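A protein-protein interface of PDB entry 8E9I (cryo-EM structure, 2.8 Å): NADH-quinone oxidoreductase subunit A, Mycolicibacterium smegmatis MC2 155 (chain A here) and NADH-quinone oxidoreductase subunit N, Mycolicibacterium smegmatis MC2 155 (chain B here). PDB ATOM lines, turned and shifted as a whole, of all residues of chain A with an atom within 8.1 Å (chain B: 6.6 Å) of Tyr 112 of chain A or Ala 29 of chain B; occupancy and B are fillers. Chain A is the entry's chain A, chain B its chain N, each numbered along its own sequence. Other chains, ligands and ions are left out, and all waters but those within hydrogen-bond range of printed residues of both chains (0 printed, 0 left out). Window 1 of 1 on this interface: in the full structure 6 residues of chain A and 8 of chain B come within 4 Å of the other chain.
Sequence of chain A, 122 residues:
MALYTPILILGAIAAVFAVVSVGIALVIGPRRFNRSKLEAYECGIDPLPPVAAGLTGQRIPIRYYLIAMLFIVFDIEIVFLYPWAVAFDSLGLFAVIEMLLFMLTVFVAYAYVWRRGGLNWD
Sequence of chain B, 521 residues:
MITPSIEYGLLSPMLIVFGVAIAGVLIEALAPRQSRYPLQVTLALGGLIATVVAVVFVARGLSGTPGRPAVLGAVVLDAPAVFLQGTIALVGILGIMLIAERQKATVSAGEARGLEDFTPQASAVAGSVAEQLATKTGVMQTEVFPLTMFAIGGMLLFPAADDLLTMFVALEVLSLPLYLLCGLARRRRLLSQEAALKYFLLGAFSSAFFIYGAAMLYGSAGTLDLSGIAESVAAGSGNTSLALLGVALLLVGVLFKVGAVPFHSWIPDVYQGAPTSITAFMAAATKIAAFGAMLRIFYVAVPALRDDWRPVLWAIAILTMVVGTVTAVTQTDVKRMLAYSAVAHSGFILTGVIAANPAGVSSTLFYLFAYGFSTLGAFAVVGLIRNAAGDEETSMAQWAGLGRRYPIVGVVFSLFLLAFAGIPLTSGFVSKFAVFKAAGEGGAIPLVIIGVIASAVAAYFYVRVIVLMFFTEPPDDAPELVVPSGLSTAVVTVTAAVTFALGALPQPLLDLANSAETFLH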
ATOM      1  N   LEU A  70      30.003  -1.542 -14.372  1.00  0.00           N
ATOM      2  CA  LEU A  70      29.076  -1.087 -15.397  1.00  0.00           C
ATOM      3  C   LEU A  70      29.772  -0.959 -16.743  1.00  0.00           C
ATOM      4  O   LEU A  70      29.161  -1.194 -17.788  1.00  0.00           O
ATOM      5  CB  LEU A  70      28.454   0.242 -14.982  1.00  0.00           C
ATOM      6  CG  LEU A  70      27.636   0.156 -13.700  1.00  0.00           C
ATOM      7  CD1 LEU A  70      27.646   1.492 -12.984  1.00  0.00           C
ATOM      8  CD2 LEU A  70      26.218  -0.291 -14.010  1.00  0.00           C
ATOM      9  N   PHE A  74      28.486  -2.462 -20.278  1.00  0.00           N
ATOM     10  CA  PHE A  74      28.124  -1.497 -21.308  1.00  0.00           C
ATOM     11  C   PHE A  74      29.034  -1.621 -22.519  1.00  0.00           C
ATOM     12  O   PHE A  74      28.563  -1.592 -23.661  1.00  0.00           O
ATOM     13  CB  PHE A  74      28.165  -0.082 -20.740  1.00  0.00           C
ATOM     14  CG  PHE A  74      26.961   0.267 -19.921  1.00  0.00           C
ATOM     15  CD1 PHE A  74      25.699   0.240 -20.482  1.00  0.00           C
ATOM     16  CD2 PHE A  74      27.088   0.616 -18.592  1.00  0.00           C
ATOM     17  CE1 PHE A  74      24.583   0.552 -19.728  1.00  0.00           C
ATOM     18  CE2 PHE A  74      25.979   0.931 -17.833  1.00  0.00           C
ATOM     19  CZ  PHE A  74      24.724   0.899 -18.404  1.00  0.00           C
ATOM     20  N   THR A 105      16.083   0.118 -23.661  1.00  0.00           N
ATOM     21  CA  THR A 105      16.359  -0.744 -22.516  1.00  0.00           C
ATOM     22  C   THR A 105      17.697  -0.386 -21.875  1.00  0.00           C
ATOM     23  O   THR A 105      17.805  -0.279 -20.644  1.00  0.00           O
ATOM     24  CB  THR A 105      16.350  -2.202 -22.965  1.00  0.00           C
ATOM     25  OG1 THR A 105      15.239  -2.429 -23.839  1.00  0.00           O
ATOM     26  CG2 THR A 105      16.237  -3.125 -21.785  1.00  0.00           C
ATOM     27  N   VAL A 106      18.720  -0.182 -22.703  1.00  0.00           N
ATOM     28  CA  VAL A 106      20.022   0.247 -22.198  1.00  0.00           C
ATOM     29  C   VAL A 106      19.895   1.588 -21.490  1.00  0.00           C
ATOM     30  O   VAL A 106      20.524   1.825 -20.455  1.00  0.00           O
ATOM     31  CB  VAL A 106      21.040   0.316 -23.347  1.00  0.00           C
ATOM     32  CG1 VAL A 106      22.342   0.941 -22.866  1.00  0.00           C
ATOM     33  CG2 VAL A 106      21.281  -1.065 -23.926  1.00  0.00           C
ATOM     34  N   PHE A 107      19.095   2.493 -22.052  1.00  0.00           N
ATOM     35  CA  PHE A 107      18.888   3.793 -21.433  1.00  0.00           C
ATOM     36  C   PHE A 107      18.230   3.649 -20.076  1.00  0.00           C
ATOM     37  O   PHE A 107      18.558   4.379 -19.141  1.00  0.00           O
ATOM     38  CB  PHE A 107      18.026   4.675 -22.331  1.00  0.00           C
ATOM     39  CG  PHE A 107      18.808   5.613 -23.188  1.00  0.00           C
ATOM     40  CD1 PHE A 107      19.526   6.651 -22.623  1.00  0.00           C
ATOM     41  CD2 PHE A 107      18.823   5.464 -24.561  1.00  0.00           C
ATOM     42  CE1 PHE A 107      20.242   7.516 -23.411  1.00  0.00           C
ATOM     43  CE2 PHE A 107      19.533   6.325 -25.351  1.00  0.00           C
ATOM     44  CZ  PHE A 107      20.246   7.355 -24.779  1.00  0.00           C
ATOM     45  N   VAL A 108      17.265   2.744 -19.959  1.00  0.00           N
ATOM     46  CA  VAL A 108      16.623   2.532 -18.669  1.00  0.00           C
ATOM     47  C   VAL A 108      17.646   2.046 -17.657  1.00  0.00           C
ATOM     48  O   VAL A 108      17.703   2.535 -16.525  1.00  0.00           O
ATOM     49  CB  VAL A 108      15.450   1.548 -18.815  1.00  0.00           C
ATOM     50  CG1 VAL A 108      14.965   1.092 -17.455  1.00  0.00           C
ATOM     51  CG2 VAL A 108      14.328   2.197 -19.591  1.00  0.00           C
ATOM     52  N   ALA A 109      18.484   1.090 -18.057  1.00  0.00           N
ATOM     53  CA  ALA A 109      19.554   0.637 -17.172  1.00  0.00           C
ATOM     54  C   ALA A 109      20.436   1.805 -16.754  1.00  0.00           C
ATOM     55  O   ALA A 109      20.758   1.981 -15.572  1.00  0.00           O
ATOM     56  CB  ALA A 109      20.388  -0.435 -17.869  1.00  0.00           C
ATOM     57  N   TYR A 110      20.827   2.625 -17.722  1.00  0.00           N
ATOM     58  CA  TYR A 110      21.750   3.720 -17.487  1.00  0.00           C
ATOM     59  C   TYR A 110      21.132   4.739 -16.545  1.00  0.00           C
ATOM     60  O   TYR A 110      21.801   5.249 -15.646  1.00  0.00           O
ATOM     61  CB  TYR A 110      22.120   4.384 -18.808  1.00  0.00           C
ATOM     62  CG  TYR A 110      23.417   5.141 -18.756  1.00  0.00           C
ATOM     63  CD1 TYR A 110      23.440   6.523 -18.806  1.00  0.00           C
ATOM     64  CD2 TYR A 110      24.623   4.469 -18.682  1.00  0.00           C
ATOM     65  CE1 TYR A 110      24.624   7.212 -18.762  1.00  0.00           C
ATOM     66  CE2 TYR A 110      25.809   5.149 -18.643  1.00  0.00           C
ATOM     67  CZ  TYR A 110      25.808   6.520 -18.687  1.00  0.00           C
ATOM     68  OH  TYR A 110      27.003   7.198 -18.647  1.00  0.00           O
ATOM     69  N   ALA A 111      19.856   5.052 -16.757  1.00  0.00           N
ATOM     70  CA  ALA A 111      19.162   6.039 -15.946  1.00  0.00           C
ATOM     71  C   ALA A 111      18.972   5.530 -14.530  1.00  0.00           C
ATOM     72  O   ALA A 111      19.058   6.295 -13.566  1.00  0.00           O
ATOM     73  CB  ALA A 111      17.814   6.383 -16.583  1.00  0.00           C
ATOM     74  N   TYR A 112      18.700   4.233 -14.384  1.00  0.00           N
ATOM     75  CA  TYR A 112      18.612   3.666 -13.046  1.00  0.00           C
ATOM     76  C   TYR A 112      19.950   3.788 -12.336  1.00  0.00           C
ATOM     77  O   TYR A 112      20.016   4.146 -11.156  1.00  0.00           O
ATOM     78  CB  TYR A 112      18.189   2.202 -13.100  1.00  0.00           C
ATOM     79  CG  TYR A 112      18.393   1.517 -11.773  1.00  0.00           C
ATOM     80  CD1 TYR A 112      17.542   1.770 -10.711  1.00  0.00           C
ATOM     81  CD2 TYR A 112      19.457   0.657 -11.562  1.00  0.00           C
ATOM     82  CE1 TYR A 112      17.723   1.164  -9.492  1.00  0.00           C
ATOM     83  CE2 TYR A 112      19.647   0.048 -10.339  1.00  0.00           C
ATOM     84  CZ  TYR A 112      18.775   0.308  -9.307  1.00  0.00           C
ATOM     85  OH  TYR A 112      18.953  -0.291  -8.087  1.00  0.00           O
ATOM     86  N   VAL A 113      21.037   3.491 -13.047  1.00  0.00           N
ATOM     87  CA  VAL A 113      22.363   3.604 -12.448  1.00  0.00           C
ATOM     88  C   VAL A 113      22.657   5.046 -12.067  1.00  0.00           C
ATOM     89  O   VAL A 113      23.186   5.323 -10.985  1.00  0.00           O
ATOM     90  CB  VAL A 113      23.429   3.057 -13.411  1.00  0.00           C
ATOM     91  CG1 VAL A 113      24.807   3.385 -12.897  1.00  0.00           C
ATOM     92  CG2 VAL A 113      23.269   1.565 -13.582  1.00  0.00           C
ATOM     93  N   TRP A 114      22.330   5.985 -12.951  1.00  0.00           N
ATOM     94  CA  TRP A 114      22.734   7.369 -12.749  1.00  0.00           C
ATOM     95  C   TRP A 114      21.887   8.032 -11.674  1.00  0.00           C
ATOM     96  O   TRP A 114      22.415   8.508 -10.663  1.00  0.00           O
ATOM     97  CB  TRP A 114      22.633   8.124 -14.072  1.00  0.00           C
ATOM     98  CG  TRP A 114      23.141   9.529 -14.044  1.00  0.00           C
ATOM     99  CD1 TRP A 114      23.507  10.257 -12.950  1.00  0.00           C
ATOM    100  CD2 TRP A 114      23.356  10.376 -15.175  1.00  0.00           C
ATOM    101  NE1 TRP A 114      23.922  11.506 -13.328  1.00  0.00           N
ATOM    102  CE2 TRP A 114      23.840  11.603 -14.692  1.00  0.00           C
ATOM    103  CE3 TRP A 114      23.178  10.218 -16.549  1.00  0.00           C
ATOM    104  CZ2 TRP A 114      24.151  12.662 -15.534  1.00  0.00           C
ATOM    105  CZ3 TRP A 114      23.486  11.270 -17.380  1.00  0.00           C
ATOM    106  CH2 TRP A 114      23.968  12.475 -16.871  1.00  0.00           C
ATOM    107  N   ARG A 115      20.568   8.067 -11.867  1.00  0.00           N
ATOM    108  CA  ARG A 115      19.711   8.775 -10.927  1.00  0.00           C
ATOM    109  C   ARG A 115      19.798   8.180  -9.529  1.00  0.00           C
ATOM    110  O   ARG A 115      19.508   8.871  -8.547  1.00  0.00           O
ATOM    111  CB  ARG A 115      18.267   8.771 -11.432  1.00  0.00           C
ATOM    112  CG  ARG A 115      17.404   9.858 -10.815  1.00  0.00           C
ATOM    113  CD  ARG A 115      16.175  10.156 -11.662  1.00  0.00           C
ATOM    114  NE  ARG A 115      15.340  11.201 -11.079  1.00  0.00           N
ATOM    115  CZ  ARG A 115      14.642  11.072  -9.958  1.00  0.00           C
ATOM    116  NH1 ARG A 115      14.630   9.939  -9.276  1.00  0.00           N
ATOM    117  NH2 ARG A 115      13.939  12.106  -9.510  1.00  0.00           N
ATOM    118  N   ARG A 116      20.197   6.917  -9.409  1.00  0.00           N
ATOM    119  CA  ARG A 116      20.393   6.295  -8.110  1.00  0.00           C
ATOM    120  C   ARG A 116      21.836   6.395  -7.630  1.00  0.00           C
ATOM    121  O   ARG A 116      22.250   5.615  -6.768  1.00  0.00           O
ATOM    122  CB  ARG A 116      19.952   4.830  -8.148  1.00  0.00           C
ATOM    123  CG  ARG A 116      18.470   4.620  -8.417  1.00  0.00           C
ATOM    124  CD  ARG A 116      17.606   5.112  -7.267  1.00  0.00           C
ATOM    125  NE  ARG A 116      17.799   4.346  -6.041  1.00  0.00           N
ATOM    126  CZ  ARG A 116      17.255   3.165  -5.794  1.00  0.00           C
ATOM    127  NH1 ARG A 116      16.464   2.570  -6.670  1.00  0.00           N
ATOM    128  NH2 ARG A 116      17.502   2.569  -4.632  1.00  0.00           N
ATOM    129  N   GLY A 117      22.614   7.318  -8.189  1.00  0.00           N
ATOM    130  CA  GLY A 117      23.931   7.631  -7.670  1.00  0.00           C
ATOM    131  C   GLY A 117      25.019   6.632  -7.983  1.00  0.00           C
ATOM    132  O   GLY A 117      26.097   6.714  -7.385  1.00  0.00           O
ATOM    133  N   GLY A 118      24.784   5.693  -8.895  1.00  0.00           N
ATOM    134  CA  GLY A 118      25.812   4.718  -9.208  1.00  0.00           C
ATOM    135  C   GLY A 118      27.061   5.344  -9.789  1.00  0.00           C
ATOM    136  O   GLY A 118      28.167   4.846  -9.573  1.00  0.00           O
ATOM    137  N   LEU A 119      26.909   6.444 -10.518  1.00  0.00           N
ATOM    138  CA  LEU A 119      28.037   7.088 -11.172  1.00  0.00           C
ATOM    139  C   LEU A 119      28.705   8.143 -10.305  1.00  0.00           C
ATOM    140  O   LEU A 119      29.645   8.795 -10.768  1.00  0.00           O
ATOM    141  CB  LEU A 119      27.575   7.736 -12.476  1.00  0.00           C
ATOM    142  CG  LEU A 119      26.808   6.808 -13.416  1.00  0.00           C
ATOM    143  CD1 LEU A 119      26.372   7.547 -14.663  1.00  0.00           C
ATOM    144  CD2 LEU A 119      27.656   5.608 -13.773  1.00  0.00           C
ATOM    145  N   GLY B  24       9.598  -1.659 -14.145  1.00  0.00           N
ATOM    146  CA  GLY B  24       9.952  -1.650 -12.736  1.00  0.00           C
ATOM    147  C   GLY B  24      11.316  -1.037 -12.497  1.00  0.00           C
ATOM    148  O   GLY B  24      11.523  -0.312 -11.521  1.00  0.00           O
ATOM    149  N   VAL B  25      12.267  -1.326 -13.382  1.00  0.00           N
ATOM    150  CA  VAL B  25      13.552  -0.647 -13.287  1.00  0.00           C
ATOM    151  C   VAL B  25      13.359   0.848 -13.480  1.00  0.00           C
ATOM    152  O   VAL B  25      14.017   1.654 -12.820  1.00  0.00           O
ATOM    153  CB  VAL B  25      14.556  -1.223 -14.298  1.00  0.00           C
ATOM    154  CG1 VAL B  25      15.849  -0.429 -14.269  1.00  0.00           C
ATOM    155  CG2 VAL B  25      14.824  -2.681 -13.991  1.00  0.00           C
ATOM    156  N   LEU B  26      12.454   1.246 -14.374  1.00  0.00           N
ATOM    157  CA  LEU B  26      12.149   2.668 -14.508  1.00  0.00           C
ATOM    158  C   LEU B  26      11.594   3.236 -13.210  1.00  0.00           C
ATOM    159  O   LEU B  26      11.948   4.349 -12.810  1.00  0.00           O
ATOM    160  CB  LEU B  26      11.155   2.898 -15.644  1.00  0.00           C
ATOM    161  CG  LEU B  26      11.753   3.080 -17.034  1.00  0.00           C
ATOM    162  CD1 LEU B  26      10.664   3.060 -18.081  1.00  0.00           C
ATOM    163  CD2 LEU B  26      12.535   4.373 -17.106  1.00  0.00           C
ATOM    164  N   ILE B  27      10.707   2.494 -12.549  1.00  0.00           N
ATOM    165  CA  ILE B  27      10.150   2.965 -11.285  1.00  0.00           C
ATOM    166  C   ILE B  27      11.264   3.159 -10.271  1.00  0.00           C
ATOM    167  O   ILE B  27      11.284   4.145  -9.526  1.00  0.00           O
ATOM    168  CB  ILE B  27       9.075   1.994 -10.761  1.00  0.00           C
ATOM    169  CG1 ILE B  27       7.914   1.860 -11.751  1.00  0.00           C
ATOM    170  CG2 ILE B  27       8.560   2.456  -9.413  1.00  0.00           C
ATOM    171  CD1 ILE B  27       7.459   3.158 -12.373  1.00  0.00           C
ATOM    172  N   GLU B  28      12.206   2.221 -10.221  1.00  0.00           N
ATOM    173  CA  GLU B  28      13.369   2.411  -9.364  1.00  0.00           C
ATOM    174  C   GLU B  28      14.155   3.649  -9.763  1.00  0.00           C
ATOM    175  O   GLU B  28      14.650   4.375  -8.895  1.00  0.00           O
ATOM    176  CB  GLU B  28      14.279   1.186  -9.420  1.00  0.00           C
ATOM    177  CG  GLU B  28      13.693  -0.052  -8.794  1.00  0.00           C
ATOM    178  CD  GLU B  28      13.198   0.201  -7.389  1.00  0.00           C
ATOM    179  OE1 GLU B  28      13.973   0.731  -6.569  1.00  0.00           O
ATOM    180  OE2 GLU B  28      12.027  -0.118  -7.106  1.00  0.00           O
ATOM    181  N   ALA B  29      14.281   3.902 -11.061  1.00  0.00           N
ATOM    182  CA  ALA B  29      15.154   4.966 -11.537  1.00  0.00           C
ATOM    183  C   ALA B  29      14.585   6.348 -11.240  1.00  0.00           C
ATOM    184  O   ALA B  29      15.298   7.222 -10.737  1.00  0.00           O
ATOM    185  CB  ALA B  29      15.396   4.807 -13.036  1.00  0.00           C
ATOM    186  N   LEU B  30      13.304   6.569 -11.544  1.00  0.00           N
ATOM    187  CA  LEU B  30      12.734   7.909 -11.506  1.00  0.00           C
ATOM    188  C   LEU B  30      11.496   8.024 -10.626  1.00  0.00           C
ATOM    189  O   LEU B  30      10.679   8.921 -10.852  1.00  0.00           O
ATOM    190  CB  LEU B  30      12.394   8.388 -12.921  1.00  0.00           C
ATOM    191  CG  LEU B  30      11.461   7.502 -13.749  1.00  0.00           C
ATOM    192  CD1 LEU B  30       9.999   7.836 -13.482  1.00  0.00           C
ATOM    193  CD2 LEU B  30      11.772   7.655 -15.223  1.00  0.00           C
ATOM    194  N   ALA B  31      11.327   7.160  -9.648  1.00  0.00           N
ATOM    195  CA  ALA B  31      10.218   7.350  -8.722  1.00  0.00           C
ATOM    196  C   ALA B  31      10.751   7.654  -7.334  1.00  0.00           C
ATOM    197  O   ALA B  31      11.794   7.107  -6.950  1.00  0.00           O
ATOM    198  CB  ALA B  31       9.333   6.109  -8.676  1.00  0.00           C
ATOM    199  N   ARG B  36       7.957   3.953  -4.306  1.00  0.00           N
ATOM    200  CA  ARG B  36       8.511   2.887  -5.134  1.00  0.00           C
ATOM    201  C   ARG B  36       7.825   1.556  -4.858  1.00  0.00           C
ATOM    202  O   ARG B  36       7.320   0.902  -5.776  1.00  0.00           O
ATOM    203  CB  ARG B  36      10.018   2.774  -4.906  1.00  0.00           C
ATOM    204  CG  ARG B  36      10.810   3.854  -5.623  1.00  0.00           C
ATOM    205  CD  ARG B  36      12.228   3.420  -5.915  1.00  0.00           C
ATOM    206  NE  ARG B  36      13.084   3.568  -4.747  1.00  0.00           N
ATOM    207  CZ  ARG B  36      13.801   4.647  -4.471  1.00  0.00           C
ATOM    208  NH1 ARG B  36      13.783   5.711  -5.256  1.00  0.00           N
ATOM    209  NH2 ARG B  36      14.552   4.662  -3.375  1.00  0.00           N
ATOM    210  N   GLU B 143      14.581  -2.788  -5.751  1.00  0.00           N
ATOM    211  CA  GLU B 143      15.137  -3.385  -6.959  1.00  0.00           C
ATOM    212  C   GLU B 143      14.849  -4.877  -7.032  1.00  0.00           C
ATOM    213  O   GLU B 143      14.929  -5.473  -8.111  1.00  0.00           O
ATOM    214  CB  GLU B 143      16.643  -3.136  -7.017  1.00  0.00           C
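The side-chain carboxylate (OE1) of Glu 28 of chain B lies within salt-bridge range of the guanidinium group (NH1) of Arg 116 of chain A.
O of Ala 29 of chain B lies within hydrogen-bond range of NH1 of Arg 115 of chain A, at 3.2 Å.
Val 106 of chain A touches none of the printed residues of chain B.
Tyr 112 of chain A touches four residues of chain B.
Of the printed residues of chain B, Arg 116 of chain A touches Glu 28 (3.1 Å) and Arg 36 (3.8 Å).
Leu 119 of chain A touches none of the printed residues of chain B.
Ala 29 of chain B touches just these residues of chain A: Ala 111 (3.9 Å), Tyr 112 (3.4 Å) and Arg 115 (3.2 Å).
Printed residues of chain A within 4 Å of Leu 30 of chain B: Arg 115.
The nearest residue of chain A that does not touch Ala 29 of chain B is Arg 116 of chain A (4.6 Å).
Val 25 of chain B touches Val 108 of chain A (CG1 to CG1, 3.6 Å).
CG2 of Val 108 of chain A touches CG of Leu 26 of chain B, at 3.7 Å.
Ala 111 of chain A touches Ala 29 of chain B (C to CB, 3.9 Å).
Tyr 112 of chain A touches Val 25 of chain B.
CB of Glu 28 of chain B touches CE1 of Tyr 112 of chain A (3.4 Å).
CA of Tyr 112 of chain A touches CB of Ala 29 of chain B (3.4 Å).
Tyr 112 of chain A touches Glu 143 of chain B.
Leu 30 of chain B touches Arg 115 of chain A (CA to NH1, 3.6 Å).
NH2 of Arg 116 of chain A touches NH2 of Arg 36 of chain B, at 3.8 Å.
Hydrophobic or aromatic side chains of chain A that line the printed part of chain B: Val 108 and Tyr 112.
Of the 10 printed residues of chain B, 7 touch a printed residue of chain A.
Hydrophobic or aromatic side chains of chain B within 4 Å of the printed part of chain A: Val 25, Leu 26 and Ala 29.
Among the printed residues, 11 pairs touch across the chains.
Among the printed residues, Asp or Glu carboxylates within 4 Å of a Lys or Arg side-chain nitrogen of the other chain: Arg 116 of chain A with Glu 28 of chain B.
The guanidinium group of Arg 36 of chain B is in salt-bridge range of the side-chain carboxylate of Glu 28 of chain B, 3.5 Å away.
The backbone carbonyl oxygen of Ala 31 of chain B is in hydrogen-bond range of the guanidinium group of Arg 36 of chain B (3.0 Å).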
